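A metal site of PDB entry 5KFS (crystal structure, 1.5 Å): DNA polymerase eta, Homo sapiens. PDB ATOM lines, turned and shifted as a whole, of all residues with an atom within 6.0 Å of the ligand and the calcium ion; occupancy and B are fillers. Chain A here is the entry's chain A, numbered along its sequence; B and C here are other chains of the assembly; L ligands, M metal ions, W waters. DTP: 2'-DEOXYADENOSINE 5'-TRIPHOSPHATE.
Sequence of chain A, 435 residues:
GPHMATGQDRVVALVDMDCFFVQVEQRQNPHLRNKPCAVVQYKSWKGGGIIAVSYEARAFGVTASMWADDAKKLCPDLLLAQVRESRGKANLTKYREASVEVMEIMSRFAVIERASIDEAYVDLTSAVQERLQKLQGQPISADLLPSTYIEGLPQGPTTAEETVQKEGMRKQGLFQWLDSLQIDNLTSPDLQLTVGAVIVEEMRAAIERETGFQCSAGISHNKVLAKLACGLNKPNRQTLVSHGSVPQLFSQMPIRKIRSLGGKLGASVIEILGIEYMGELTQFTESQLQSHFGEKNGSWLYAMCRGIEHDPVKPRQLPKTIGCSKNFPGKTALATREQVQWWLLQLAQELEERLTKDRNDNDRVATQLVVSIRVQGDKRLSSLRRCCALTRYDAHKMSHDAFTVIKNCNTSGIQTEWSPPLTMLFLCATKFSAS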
ATOM      1  N   ASP A  16       3.345 -13.245  -1.805  1.00  0.00           N
ATOM      2  CA  ASP A  16       2.838 -12.962  -3.149  1.00  0.00           C
ATOM      3  C   ASP A  16       3.687 -13.746  -4.139  1.00  0.00           C
ATOM      4  O   ASP A  16       4.875 -13.441  -4.313  1.00  0.00           O
ATOM      5  CB  ASP A  16       2.950 -11.443  -3.409  1.00  0.00           C
ATOM      6  CG  ASP A  16       2.225 -10.980  -4.647  1.00  0.00           C
ATOM      7  OD1 ASP A  16       1.913  -9.759  -4.723  1.00  0.00           O
ATOM      8  OD2 ASP A  16       1.990 -11.785  -5.561  1.00  0.00           O
ATOM      9  N   MET A  17       3.112 -14.750  -4.811  1.00  0.00           N
ATOM     10  CA  MET A  17       3.864 -15.546  -5.778  1.00  0.00           C
ATOM     11  C   MET A  17       4.383 -14.657  -6.929  1.00  0.00           C
ATOM     12  O   MET A  17       3.743 -13.787  -7.368  1.00  0.00           O
ATOM     13  CB  MET A  17       3.037 -16.733  -6.341  1.00  0.00           C
ATOM     14  CG  MET A  17       2.366 -17.605  -5.287  1.00  0.00           C
ATOM     15  SD  MET A  17       3.510 -18.336  -4.069  1.00  0.00           S
ATOM     16  CE  MET A  17       4.481 -19.376  -5.105  1.00  0.00           C
ATOM     17  N   ASP A  18       5.581 -14.955  -7.376  1.00  0.00           N
ATOM     18  CA  ASP A  18       6.139 -14.175  -8.473  1.00  0.00           C
ATOM     19  C   ASP A  18       5.593 -14.683  -9.801  1.00  0.00           C
ATOM     20  O   ASP A  18       5.496 -15.860  -9.977  1.00  0.00           O
ATOM     21  CB  ASP A  18       7.651 -14.267  -8.483  1.00  0.00           C
ATOM     22  CG  ASP A  18       8.295 -13.677  -7.238  1.00  0.00           C
ATOM     23  OD1 ASP A  18       7.799 -12.750  -6.700  1.00  0.00           O
ATOM     24  OD2 ASP A  18       9.295 -14.187  -6.930  1.00  0.00           O
ATOM     25  N   CYS A  19       5.141 -13.766 -10.641  1.00  0.00           N
ATOM     26  CA  CYS A  19       4.661 -14.080 -11.992  1.00  0.00           C
ATOM     27  C   CYS A  19       3.861 -15.390 -12.045  1.00  0.00           C
ATOM     28  O   CYS A  19       4.282 -16.276 -12.725  1.00  0.00           O
ATOM     29  CB  CYS A  19       5.691 -13.893 -13.099  1.00  0.00           C
ATOM     30  SG  CYS A  19       7.215 -14.892 -12.959  1.00  0.00           S
ATOM     31  N   PHE A  20       2.821 -15.530 -11.258  1.00  0.00           N
ATOM     32  CA  PHE A  20       2.348 -16.818 -10.845  1.00  0.00           C
ATOM     33  C   PHE A  20       1.915 -17.745 -11.972  1.00  0.00           C
ATOM     34  O   PHE A  20       2.405 -18.825 -12.036  1.00  0.00           O
ATOM     35  CB  PHE A  20       1.202 -16.684  -9.845  1.00  0.00           C
ATOM     36  CG  PHE A  20       0.735 -18.004  -9.287  1.00  0.00           C
ATOM     37  CD1 PHE A  20       1.633 -18.872  -8.746  1.00  0.00           C
ATOM     38  CD2 PHE A  20      -0.585 -18.394  -9.305  1.00  0.00           C
ATOM     39  CE1 PHE A  20       1.225 -20.092  -8.255  1.00  0.00           C
ATOM     40  CE2 PHE A  20      -0.985 -19.622  -8.769  1.00  0.00           C
ATOM     41  CZ  PHE A  20      -0.088 -20.448  -8.252  1.00  0.00           C
ATOM     42  N   PHE A  21       1.098 -17.283 -12.878  1.00  0.00           N
ATOM     43  CA  PHE A  21       0.659 -18.226 -13.917  1.00  0.00           C
ATOM     44  C   PHE A  21       1.835 -18.640 -14.807  1.00  0.00           C
ATOM     45  O   PHE A  21       1.854 -19.750 -15.313  1.00  0.00           O
ATOM     46  CB  PHE A  21      -0.450 -17.642 -14.795  1.00  0.00           C
ATOM     47  CG  PHE A  21      -1.791 -17.497 -14.131  1.00  0.00           C
ATOM     48  CD1 PHE A  21      -1.964 -17.549 -12.754  1.00  0.00           C
ATOM     49  CD2 PHE A  21      -2.897 -17.258 -14.917  1.00  0.00           C
ATOM     50  CE1 PHE A  21      -3.232 -17.411 -12.180  1.00  0.00           C
ATOM     51  CE2 PHE A  21      -4.166 -17.098 -14.356  1.00  0.00           C
ATOM     52  CZ  PHE A  21      -4.324 -17.155 -12.986  1.00  0.00           C
ATOM     53  N   VAL A  22       2.795 -17.728 -15.007  1.00  0.00           N
ATOM     54  CA  VAL A  22       4.002 -18.063 -15.756  1.00  0.00           C
ATOM     55  C   VAL A  22       4.786 -19.173 -15.041  1.00  0.00           C
ATOM     56  O   VAL A  22       5.211 -20.140 -15.698  1.00  0.00           O
ATOM     57  CB  VAL A  22       4.903 -16.832 -15.976  1.00  0.00           C
ATOM     58  CG1 VAL A  22       6.319 -17.238 -16.355  1.00  0.00           C
ATOM     59  CG2 VAL A  22       4.289 -15.916 -17.030  1.00  0.00           C
ATOM     60  N   GLN A  41      -4.532 -15.608 -22.946  1.00  0.00           N
ATOM     61  CA  GLN A  41      -5.809 -16.290 -23.071  1.00  0.00           C
ATOM     62  C   GLN A  41      -6.438 -15.971 -24.411  1.00  0.00           C
ATOM     63  O   GLN A  41      -6.477 -14.808 -24.812  1.00  0.00           O
ATOM     64  CB  GLN A  41      -6.762 -15.941 -21.917  1.00  0.00           C
ATOM     65  CG  GLN A  41      -6.861 -14.489 -21.534  1.00  0.00           C
ATOM     66  CD  GLN A  41      -7.732 -14.301 -20.295  1.00  0.00           C
ATOM     67  OE1 GLN A  41      -8.087 -15.271 -19.616  1.00  0.00           O
ATOM     68  NE2 GLN A  41      -8.099 -13.066 -20.015  1.00  0.00           N
ATOM     69  N   ILE A  51      -1.945 -12.218 -19.714  1.00  0.00           N
ATOM     70  CA  ILE A  51      -2.364 -12.044 -18.332  1.00  0.00           C
ATOM     71  C   ILE A  51      -1.256 -12.280 -17.296  1.00  0.00           C
ATOM     72  O   ILE A  51      -1.457 -11.978 -16.130  1.00  0.00           O
ATOM     73  CB  ILE A  51      -3.567 -12.950 -17.986  1.00  0.00           C
ATOM     74  CG1 ILE A  51      -3.237 -14.454 -18.135  1.00  0.00           C
ATOM     75  CG2 ILE A  51      -4.772 -12.552 -18.826  1.00  0.00           C
ATOM     76  CD1 ILE A  51      -4.348 -15.366 -17.602  1.00  0.00           C
ATOM     77  N   ALA A  52      -0.102 -12.770 -17.717  1.00  0.00           N
ATOM     78  CA  ALA A  52       1.053 -12.891 -16.805  1.00  0.00           C
ATOM     79  C   ALA A  52       2.355 -12.865 -17.605  1.00  0.00           C
ATOM     80  O   ALA A  52       2.373 -13.340 -18.742  1.00  0.00           O
ATOM     81  CB  ALA A  52       0.966 -14.166 -15.951  1.00  0.00           C
ATOM     82  N   VAL A  53       3.423 -12.310 -17.029  1.00  0.00           N
ATOM     83  CA  VAL A  53       4.666 -12.027 -17.750  1.00  0.00           C
ATOM     84  C   VAL A  53       5.896 -12.328 -16.897  1.00  0.00           C
ATOM     85  O   VAL A  53       5.986 -11.843 -15.762  1.00  0.00           O
ATOM     86  CB  VAL A  53       4.726 -10.540 -18.201  1.00  0.00           C
ATOM     87  CG1 VAL A  53       5.942 -10.278 -19.070  1.00  0.00           C
ATOM     88  CG2 VAL A  53       3.477 -10.156 -18.949  1.00  0.00           C
ATOM     89  N   TYR A  55       9.798 -12.180 -15.605  1.00  0.00           N
ATOM     90  CA  TYR A  55      10.616 -10.997 -15.360  1.00  0.00           C
ATOM     91  C   TYR A  55      11.600 -10.751 -16.509  1.00  0.00           C
ATOM     92  O   TYR A  55      11.883  -9.588 -16.838  1.00  0.00           O
ATOM     93  CB  TYR A  55      11.335 -11.112 -13.999  1.00  0.00           C
ATOM     94  CG  TYR A  55      10.378 -10.762 -12.879  1.00  0.00           C
ATOM     95  CD1 TYR A  55       9.428 -11.673 -12.424  1.00  0.00           C
ATOM     96  CD2 TYR A  55      10.331  -9.477 -12.361  1.00  0.00           C
ATOM     97  CE1 TYR A  55       8.508 -11.339 -11.460  1.00  0.00           C
ATOM     98  CE2 TYR A  55       9.423  -9.132 -11.393  1.00  0.00           C
ATOM     99  CZ  TYR A  55       8.506 -10.058 -10.942  1.00  0.00           C
ATOM    100  OH  TYR A  55       7.593  -9.697  -9.979  1.00  0.00           O
ATOM    101  N   ARG A  58       9.517  -8.863 -18.918  1.00  0.00           N
ATOM    102  CA  ARG A  58       9.240  -7.504 -18.460  1.00  0.00           C
ATOM    103  C   ARG A  58      10.384  -6.548 -18.805  1.00  0.00           C
ATOM    104  O   ARG A  58      10.146  -5.366 -19.030  1.00  0.00           O
ATOM    105  CB  ARG A  58       8.981  -7.466 -16.956  1.00  0.00           C
ATOM    106  CG  ARG A  58       7.782  -8.282 -16.542  1.00  0.00           C
ATOM    107  CD  ARG A  58       7.555  -8.179 -15.049  1.00  0.00           C
ATOM    108  NE  ARG A  58       6.629  -9.213 -14.625  1.00  0.00           N
ATOM    109  CZ  ARG A  58       6.030  -9.267 -13.445  1.00  0.00           C
ATOM    110  NH1 ARG A  58       6.257  -8.314 -12.543  1.00  0.00           N
ATOM    111  NH2 ARG A  58       5.199 -10.278 -13.161  1.00  0.00           N
ATOM    112  N   SER A 116      -6.001 -13.564  -2.675  1.00  0.00           N
ATOM    113  CA  SER A 116      -6.215 -13.735  -4.112  1.00  0.00           C
ATOM    114  C   SER A 116      -5.725 -15.105  -4.498  1.00  0.00           C
ATOM    115  O   SER A 116      -5.310 -15.888  -3.643  1.00  0.00           O
ATOM    116  CB  SER A 116      -5.471 -12.681  -4.916  1.00  0.00           C
ATOM    117  OG  SER A 116      -4.077 -12.938  -4.840  1.00  0.00           O
ATOM    118  N   ILE A 117      -5.710 -15.390  -5.805  1.00  0.00           N
ATOM    119  CA  ILE A 117      -5.258 -16.703  -6.245  1.00  0.00           C
ATOM    120  C   ILE A 117      -3.788 -16.987  -5.858  1.00  0.00           C
ATOM    121  O   ILE A 117      -3.407 -18.134  -5.709  1.00  0.00           O
ATOM    122  CB  ILE A 117      -5.451 -16.860  -7.778  1.00  0.00           C
ATOM    123  CG1 ILE A 117      -5.398 -18.338  -8.172  1.00  0.00           C
ATOM    124  CG2 ILE A 117      -4.465 -15.992  -8.522  1.00  0.00           C
ATOM    125  CD1 ILE A 117      -5.973 -18.645  -9.558  1.00  0.00           C
ATOM    126  N   ASP A 118      -2.979 -15.942  -5.651  1.00  0.00           N
ATOM    127  CA  ASP A 118      -1.557 -16.183  -5.369  1.00  0.00           C
ATOM    128  C   ASP A 118      -0.991 -15.324  -4.234  1.00  0.00           C
ATOM    129  O   ASP A 118       0.220 -15.171  -4.112  1.00  0.00           O
ATOM    130  CB  ASP A 118      -0.733 -15.976  -6.643  1.00  0.00           C
ATOM    131  CG  ASP A 118      -0.457 -14.518  -6.929  1.00  0.00           C
ATOM    132  OD1 ASP A 118       0.645 -14.229  -7.458  1.00  0.00           O
ATOM    133  OD2 ASP A 118      -1.311 -13.674  -6.596  1.00  0.00           O
ATOM    134  N   GLU A 119      -1.885 -14.784  -3.404  1.00  0.00           N
ATOM    135  CA  GLU A 119      -1.499 -13.961  -2.252  1.00  0.00           C
ATOM    136  C   GLU A 119      -2.162 -14.448  -1.001  1.00  0.00           C
ATOM    137  O   GLU A 119      -3.352 -14.745  -1.007  1.00  0.00           O
ATOM    138  CB  GLU A 119      -1.896 -12.498  -2.438  1.00  0.00           C
ATOM    139  CG  GLU A 119      -1.011 -11.716  -3.348  1.00  0.00           C
ATOM    140  CD  GLU A 119      -1.447 -10.276  -3.430  1.00  0.00           C
ATOM    141  OE1 GLU A 119      -2.642 -10.037  -3.682  1.00  0.00           O
ATOM    142  OE2 GLU A 119      -0.607  -9.383  -3.214  1.00  0.00           O
ATOM    143  N   LYS A 234      11.119  -7.291  -5.447  1.00  0.00           N
ATOM    144  CA  LYS A 234      10.484  -8.440  -6.110  1.00  0.00           C
ATOM    145  C   LYS A 234      11.354  -8.588  -7.268  1.00  0.00           C
ATOM    146  O   LYS A 234      11.832  -7.587  -7.719  1.00  0.00           O
ATOM    147  CB  LYS A 234       9.111  -8.069  -6.638  1.00  0.00           C
ATOM    148  CG  LYS A 234       7.909  -8.595  -5.919  1.00  0.00           C
ATOM    149  CD  LYS A 234       6.690  -8.983  -6.828  1.00  0.00           C
ATOM    150  CE  LYS A 234       5.567  -9.732  -6.128  1.00  0.00           C
ATOM    151  NZ  LYS A 234       5.548 -11.222  -6.356  1.00  0.00           N
ATOM    152  N   PRO A 235      11.641  -9.769  -7.759  1.00  0.00           N
ATOM    153  CA  PRO A 235      11.057 -11.028  -7.281  1.00  0.00           C
ATOM    154  C   PRO A 235      11.996 -11.796  -6.357  1.00  0.00           C
ATOM    155  O   PRO A 235      13.173 -11.437  -6.198  1.00  0.00           O
ATOM    156  CB  PRO A 235      10.853 -11.799  -8.573  1.00  0.00           C
ATOM    157  CG  PRO A 235      12.087 -11.401  -9.399  1.00  0.00           C
ATOM    158  CD  PRO A 235      12.377  -9.963  -9.029  1.00  0.00           C
ATOM    159  P    DT B   3      -9.708  -2.958 -25.616  1.00  0.00           P
ATOM    160  OP1  DT B   3     -10.408  -1.732 -26.041  1.00  0.00           O
ATOM    161  OP2  DT B   3      -8.244  -3.074 -25.760  1.00  0.00           O
ATOM    162  O5'  DT B   3     -10.085  -3.239 -24.088  1.00  0.00           O
ATOM    163  C5'  DT B   3      -9.216  -4.016 -23.272  1.00  0.00           C
ATOM    164  C4'  DT B   3      -9.380  -5.496 -23.570  1.00  0.00           C
ATOM    165  O4'  DT B   3      -8.279  -6.221 -22.963  1.00  0.00           O
ATOM    166  C3'  DT B   3     -10.648  -6.123 -23.021  1.00  0.00           C
ATOM    167  O3'  DT B   3     -11.095  -7.166 -23.878  1.00  0.00           O
ATOM    168  C2'  DT B   3     -10.189  -6.670 -21.674  1.00  0.00           C
ATOM    169  C1'  DT B   3      -8.784  -7.144 -22.016  1.00  0.00           C
ATOM    170  N1   DT B   3      -7.867  -7.153 -20.843  1.00  0.00           N
ATOM    171  C2   DT B   3      -7.160  -8.306 -20.531  1.00  0.00           C
ATOM    172  O2   DT B   3      -7.237  -9.327 -21.183  1.00  0.00           O
ATOM    173  N3   DT B   3      -6.353  -8.197 -19.427  1.00  0.00           N
ATOM    174  C4   DT B   3      -6.184  -7.090 -18.613  1.00  0.00           C
ATOM    175  O4   DT B   3      -5.434  -7.097 -17.641  1.00  0.00           O
ATOM    176  C5   DT B   3      -6.956  -5.924 -18.993  1.00  0.00           C
ATOM    177  C7   DT B   3      -6.851  -4.657 -18.191  1.00  0.00           C
ATOM    178  C6   DT B   3      -7.745  -6.007 -20.076  1.00  0.00           C
ATOM    179  P    DT B   4     -12.333  -8.088 -23.434  1.00  0.00           P
ATOM    180  OP1  DT B   4     -12.866  -8.761 -24.639  1.00  0.00           O
ATOM    181  OP2  DT B   4     -13.229  -7.277 -22.578  1.00  0.00           O
ATOM    182  O5'  DT B   4     -11.679  -9.186 -22.482  1.00  0.00           O
ATOM    183  C5'  DT B   4     -10.969 -10.267 -23.044  1.00  0.00           C
ATOM    184  C4'  DT B   4     -10.921 -11.416 -22.069  1.00  0.00           C
ATOM    185  O4'  DT B   4     -10.055 -11.081 -20.964  1.00  0.00           O
ATOM    186  C3'  DT B   4     -12.257 -11.797 -21.428  1.00  0.00           C
ATOM    187  O3'  DT B   4     -12.272 -13.184 -21.268  1.00  0.00           O
ATOM    188  C2'  DT B   4     -12.217 -11.058 -20.087  1.00  0.00           C
ATOM    189  C1'  DT B   4     -10.748 -11.206 -19.748  1.00  0.00           C
ATOM    190  N1   DT B   4     -10.198 -10.198 -18.800  1.00  0.00           N
ATOM    191  C2   DT B   4      -9.262 -10.617 -17.903  1.00  0.00           C
ATOM    192  O2   DT B   4      -8.903 -11.769 -17.822  1.00  0.00           O
ATOM    193  N3   DT B   4      -8.767  -9.631 -17.093  1.00  0.00           N
ATOM    194  C4   DT B   4      -9.088  -8.295 -17.088  1.00  0.00           C
ATOM    195  O4   DT B   4      -8.580  -7.496 -16.312  1.00  0.00           O
ATOM    196  C5   DT B   4     -10.072  -7.906 -18.077  1.00  0.00           C
ATOM    197  C7   DT B   4     -10.515  -6.472 -18.169  1.00  0.00           C
ATOM    198  C6   DT B   4     -10.568  -8.862 -18.894  1.00  0.00           C
ATOM    199  P    DA B   5     -13.523 -13.948 -20.616  1.00  0.00           P
ATOM    200  OP1  DA B   5     -13.687 -15.200 -21.370  1.00  0.00           O
ATOM    201  OP2  DA B   5     -14.645 -13.018 -20.437  1.00  0.00           O
ATOM    202  O5'  DA B   5     -13.001 -14.302 -19.140  1.00  0.00           O
ATOM    203  C5'  DA B   5     -11.931 -15.205 -18.963  1.00  0.00           C
ATOM    204  C4'  DA B   5     -11.678 -15.428 -17.496  1.00  0.00           C
ATOM    205  O4'  DA B   5     -11.086 -14.242 -16.909  1.00  0.00           O
ATOM    206  C3'  DA B   5     -12.931 -15.734 -16.663  1.00  0.00           C
ATOM    207  O3'  DA B   5     -12.615 -16.736 -15.694  1.00  0.00           O
ATOM    208  C2'  DA B   5     -13.214 -14.386 -15.988  1.00  0.00           C
ATOM    209  C1'  DA B   5     -11.789 -13.922 -15.733  1.00  0.00           C
ATOM    210  N9   DA B   5     -11.661 -12.487 -15.471  1.00  0.00           N
ATOM    211  C8   DA B   5     -12.356 -11.473 -16.068  1.00  0.00           C
ATOM    212  N7   DA B   5     -12.014 -10.284 -15.637  1.00  0.00           N
ATOM    213  C5   DA B   5     -11.034 -10.529 -14.690  1.00  0.00           C
ATOM    214  C6   DA B   5     -10.270  -9.673 -13.870  1.00  0.00           C
ATOM    215  N6   DA B   5     -10.398  -8.340 -13.878  1.00  0.00           N
ATOM    216  N1   DA B   5      -9.372 -10.246 -13.048  1.00  0.00           N
ATOM    217  C2   DA B   5      -9.252 -11.577 -13.046  1.00  0.00           C
ATOM    218  N3   DA B   5      -9.902 -12.478 -13.774  1.00  0.00           N
ATOM    219  C4   DA B   5     -10.800 -11.876 -14.585  1.00  0.00           C
ATOM    220  P    DT C   8      -3.542  -5.727  -6.629  1.00  0.00           P
ATOM    221  OP1  DT C   8      -2.287  -5.717  -5.847  1.00  0.00           O
ATOM    222  OP2  DT C   8      -3.597  -5.020  -7.929  1.00  0.00           O
ATOM    223  O5'  DT C   8      -4.029  -7.246  -6.927  1.00  0.00           O
ATOM    224  C5'  DT C   8      -3.733  -8.304  -6.007  1.00  0.00           C
ATOM    225  C4'  DT C   8      -4.223  -9.657  -6.529  1.00  0.00           C
ATOM    226  O4'  DT C   8      -5.471  -9.483  -7.232  1.00  0.00           O
ATOM    227  C3'  DT C   8      -3.294 -10.400  -7.500  1.00  0.00           C
ATOM    228  O3'  DT C   8      -3.258 -11.763  -7.173  1.00  0.00           O
ATOM    229  C2'  DT C   8      -3.930 -10.168  -8.862  1.00  0.00           C
ATOM    230  C1'  DT C   8      -5.406 -10.098  -8.506  1.00  0.00           C
ATOM    231  N1   DT C   8      -6.205  -9.285  -9.454  1.00  0.00           N
ATOM    232  C2   DT C   8      -7.055  -9.927 -10.330  1.00  0.00           C
ATOM    233  O2   DT C   8      -7.171 -11.139 -10.381  1.00  0.00           O
ATOM    234  N3   DT C   8      -7.761  -9.081 -11.162  1.00  0.00           N
ATOM    235  C4   DT C   8      -7.689  -7.710 -11.200  1.00  0.00           C
ATOM    236  O4   DT C   8      -8.365  -7.043 -11.987  1.00  0.00           O
ATOM    237  C5   DT C   8      -6.774  -7.110 -10.268  1.00  0.00           C
ATOM    238  C7   DT C   8      -6.640  -5.612 -10.222  1.00  0.00           C
ATOM    239  C6   DT C   8      -6.090  -7.916  -9.446  1.00  0.00           C
HETATM  240  PG  DTP L   1       4.099 -10.410  -9.795  1.00  0.00           P
HETATM  241  O1G DTP L   1       3.318 -10.643  -8.526  1.00  0.00           O
HETATM  242  O2G DTP L   1       5.420 -11.109  -9.739  1.00  0.00           O
HETATM  243  O3G DTP L   1       4.286  -8.935 -10.146  1.00  0.00           O
HETATM  244  PB  DTP L   1       1.962 -11.897 -11.072  1.00  0.00           P
HETATM  245  O1B DTP L   1       1.977 -12.930  -9.972  1.00  0.00           O
HETATM  246  O2B DTP L   1       1.823 -12.476 -12.466  1.00  0.00           O
HETATM  247  O3B DTP L   1       3.327 -11.029 -11.053  1.00  0.00           O
HETATM  248  PA  DTP L   1      -0.350 -10.723  -9.813  1.00  0.00           P
HETATM  249  O1A DTP L   1       0.167 -10.985  -8.460  1.00  0.00           O
HETATM  250  O2A DTP L   1      -0.972  -9.360 -10.010  1.00  0.00           O
HETATM  251  O3A DTP L   1       0.819 -10.815 -10.881  1.00  0.00           O
HETATM  252  O5' DTP L   1      -1.456 -11.764 -10.239  1.00  0.00           O
HETATM  253  C5' DTP L   1      -1.360 -13.130  -9.977  1.00  0.00           C
HETATM  254  C4' DTP L   1      -1.887 -13.920 -11.176  1.00  0.00           C
HETATM  255  O4' DTP L   1      -3.265 -13.611 -11.301  1.00  0.00           O
HETATM  256  C3' DTP L   1      -1.244 -13.575 -12.446  1.00  0.00           C
HETATM  257  O3' DTP L   1      -0.104 -14.418 -12.686  1.00  0.00           O
HETATM  258  C2' DTP L   1      -2.315 -13.777 -13.446  1.00  0.00           C
HETATM  259  C1' DTP L   1      -3.561 -13.461 -12.698  1.00  0.00           C
HETATM  260  N9  DTP L   1      -4.053 -12.145 -12.916  1.00  0.00           N
HETATM  261  C8  DTP L   1      -3.654 -10.999 -12.311  1.00  0.00           C
HETATM  262  N7  DTP L   1      -4.346  -9.958 -12.758  1.00  0.00           N
HETATM  263  C5  DTP L   1      -5.242 -10.408 -13.665  1.00  0.00           C
HETATM  264  C6  DTP L   1      -6.222  -9.822 -14.460  1.00  0.00           C
HETATM  265  N6  DTP L   1      -6.463  -8.417 -14.425  1.00  0.00           N
HETATM  266  N1  DTP L   1      -6.931 -10.590 -15.282  1.00  0.00           N
HETATM  267  C2  DTP L   1      -6.763 -11.921 -15.366  1.00  0.00           C
HETATM  268  N3  DTP L   1      -5.817 -12.530 -14.602  1.00  0.00           N
HETATM  269  C4  DTP L   1      -5.067 -11.793 -13.762  1.00  0.00           C
HETATM  270 CA    CA M   1       1.942 -12.346  -7.718  1.00  0.00          CA
HETATM  271  O   HOH W   1      -6.876 -15.089 -14.339  1.00  0.00           O
HETATM  272  O   HOH W   2       0.537  -6.929 -10.420  1.00  0.00           O
HETATM  273  O   HOH W   3       2.948  -7.351  -8.158  1.00  0.00           O
HETATM  274  O   HOH W   4      -0.806  -8.612 -13.217  1.00  0.00           O
HETATM  275  O   HOH W   5       0.834  -8.795  -6.930  1.00  0.00           O
HETATM  276  O   HOH W   6       2.796  -7.472 -11.860  1.00  0.00           O
HETATM  277  O   HOH W   7      -2.591  -9.761 -15.036  1.00  0.00           O
HETATM  278  O   HOH W   8      -6.091 -13.408 -10.438  1.00  0.00           O
HETATM  279  O   HOH W   9       2.773 -11.097 -14.579  1.00  0.00           O
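The backbone NH (N) of Cys 19 lies within hydrogen-bond range of an oxygen (O2G) of the ligand, 2.8 Å away.
The side-chain amino group (NZ) of Lys 234 is in salt-bridge range of an oxygen (O2G) of the ligand, 3.4 Å away.
O2B of the ligand is in hydrogen-bond range of N of Phe 20 (3.4 Å).
O4 of DT 8 of chain C lies within hydrogen-bond range of a nitrogen (N6) of the ligand (3.4 Å).
The guanidinium group of Arg 58 is in salt-bridge range of an oxygen (O3G) of the ligand (3.2 Å).
A nitrogen (N6) of the ligand sits at hydrogen-bond distance from O4 of DT 4 of chain B, at 3.0 Å.
The side-chain hydroxyl (OH) of Tyr 55 sits at hydrogen-bond distance from an oxygen (O2G) of the ligand (2.6 Å).
The backbone NH of Phe 21 sits at hydrogen-bond distance from an oxygen (O3') of the ligand (3.1 Å).
The backbone carbonyl oxygen (O) of Val 53 is in hydrogen-bond range of the guanidinium group (NE) of Arg 58 (2.9 Å).
The side-chain amino group (NZ) of Lys 234 lies within salt-bridge range of the side-chain carboxylate (OD1) of Asp 18 (2.7 Å).
The guanidinium group (NH1) of Arg 58 sits at hydrogen-bond distance from the side-chain hydroxyl (OH) of Tyr 55 (3.2 Å).
The side-chain hydroxyl of Ser 116 is in hydrogen-bond range of O3' of DT 8 of chain C (2.7 Å).
O of Met 17 lies close to NZ of Lys 234 (3.3 Å).
The backbone carbonyl oxygen of Asp 16 is in hydrogen-bond range of the side-chain amino group of Lys 234 (3.1 Å).
The side-chain amide nitrogen (NE2) of Gln 41 lies within hydrogen-bond range of O2 of DT 4 of chain B, at 2.7 Å.
OG of Ser 116 sits close to N of Asp 118 (3.3 Å).
N1 of DA 5 of chain B sits close to N1 of the ligand (3.3 Å).
Merely in contact with the ligand: Ile 51 (3.3 Å), Asp 18 (3.4 Å), Ala 52 (3.4 Å), DT 3 of chain B (3.6 Å) and Ile 117 (3.9 Å).
Hydrophobic or aromatic side chains that line the ligand: Phe 20, Phe 21, Ala 52, Tyr 55 and Ile 117.
Within 4 Å of the calcium ion: Asp 16, Met 17 and Asp 118.
The nearest printed residue that does not touch the calcium ion is Lys 234 (4.02 Å).
The calcium ion is bound by the side-chain carboxylate of Asp 16 (2.2 Å), the side-chain carboxylate of Asp 118 (2.3 Å), an oxygen (O1B) of the ligand (2.3 Å), the backbone carbonyl oxygen of Met 17 (2.3 Å), an oxygen (O1G) of the ligand (2.3 Å) and an oxygen (O1A) of the ligand (2.4 Å).
The calcium ion has six donor atoms within binding distance.
Water W9 lies within hydrogen-bond range of O2B of the ligand, N of Val 53 and NH2 of Arg 58.
Water W7 lies within hydrogen-bond range of the backbone carbonyl oxygen of Ile 51 (2.7 Å) and a nitrogen (N7) of the ligand (2.9 Å).
Water W8 bridges O2 of DT 8 of chain C (2.5 Å) and an oxygen (O4') of the ligand (3.0 Å).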
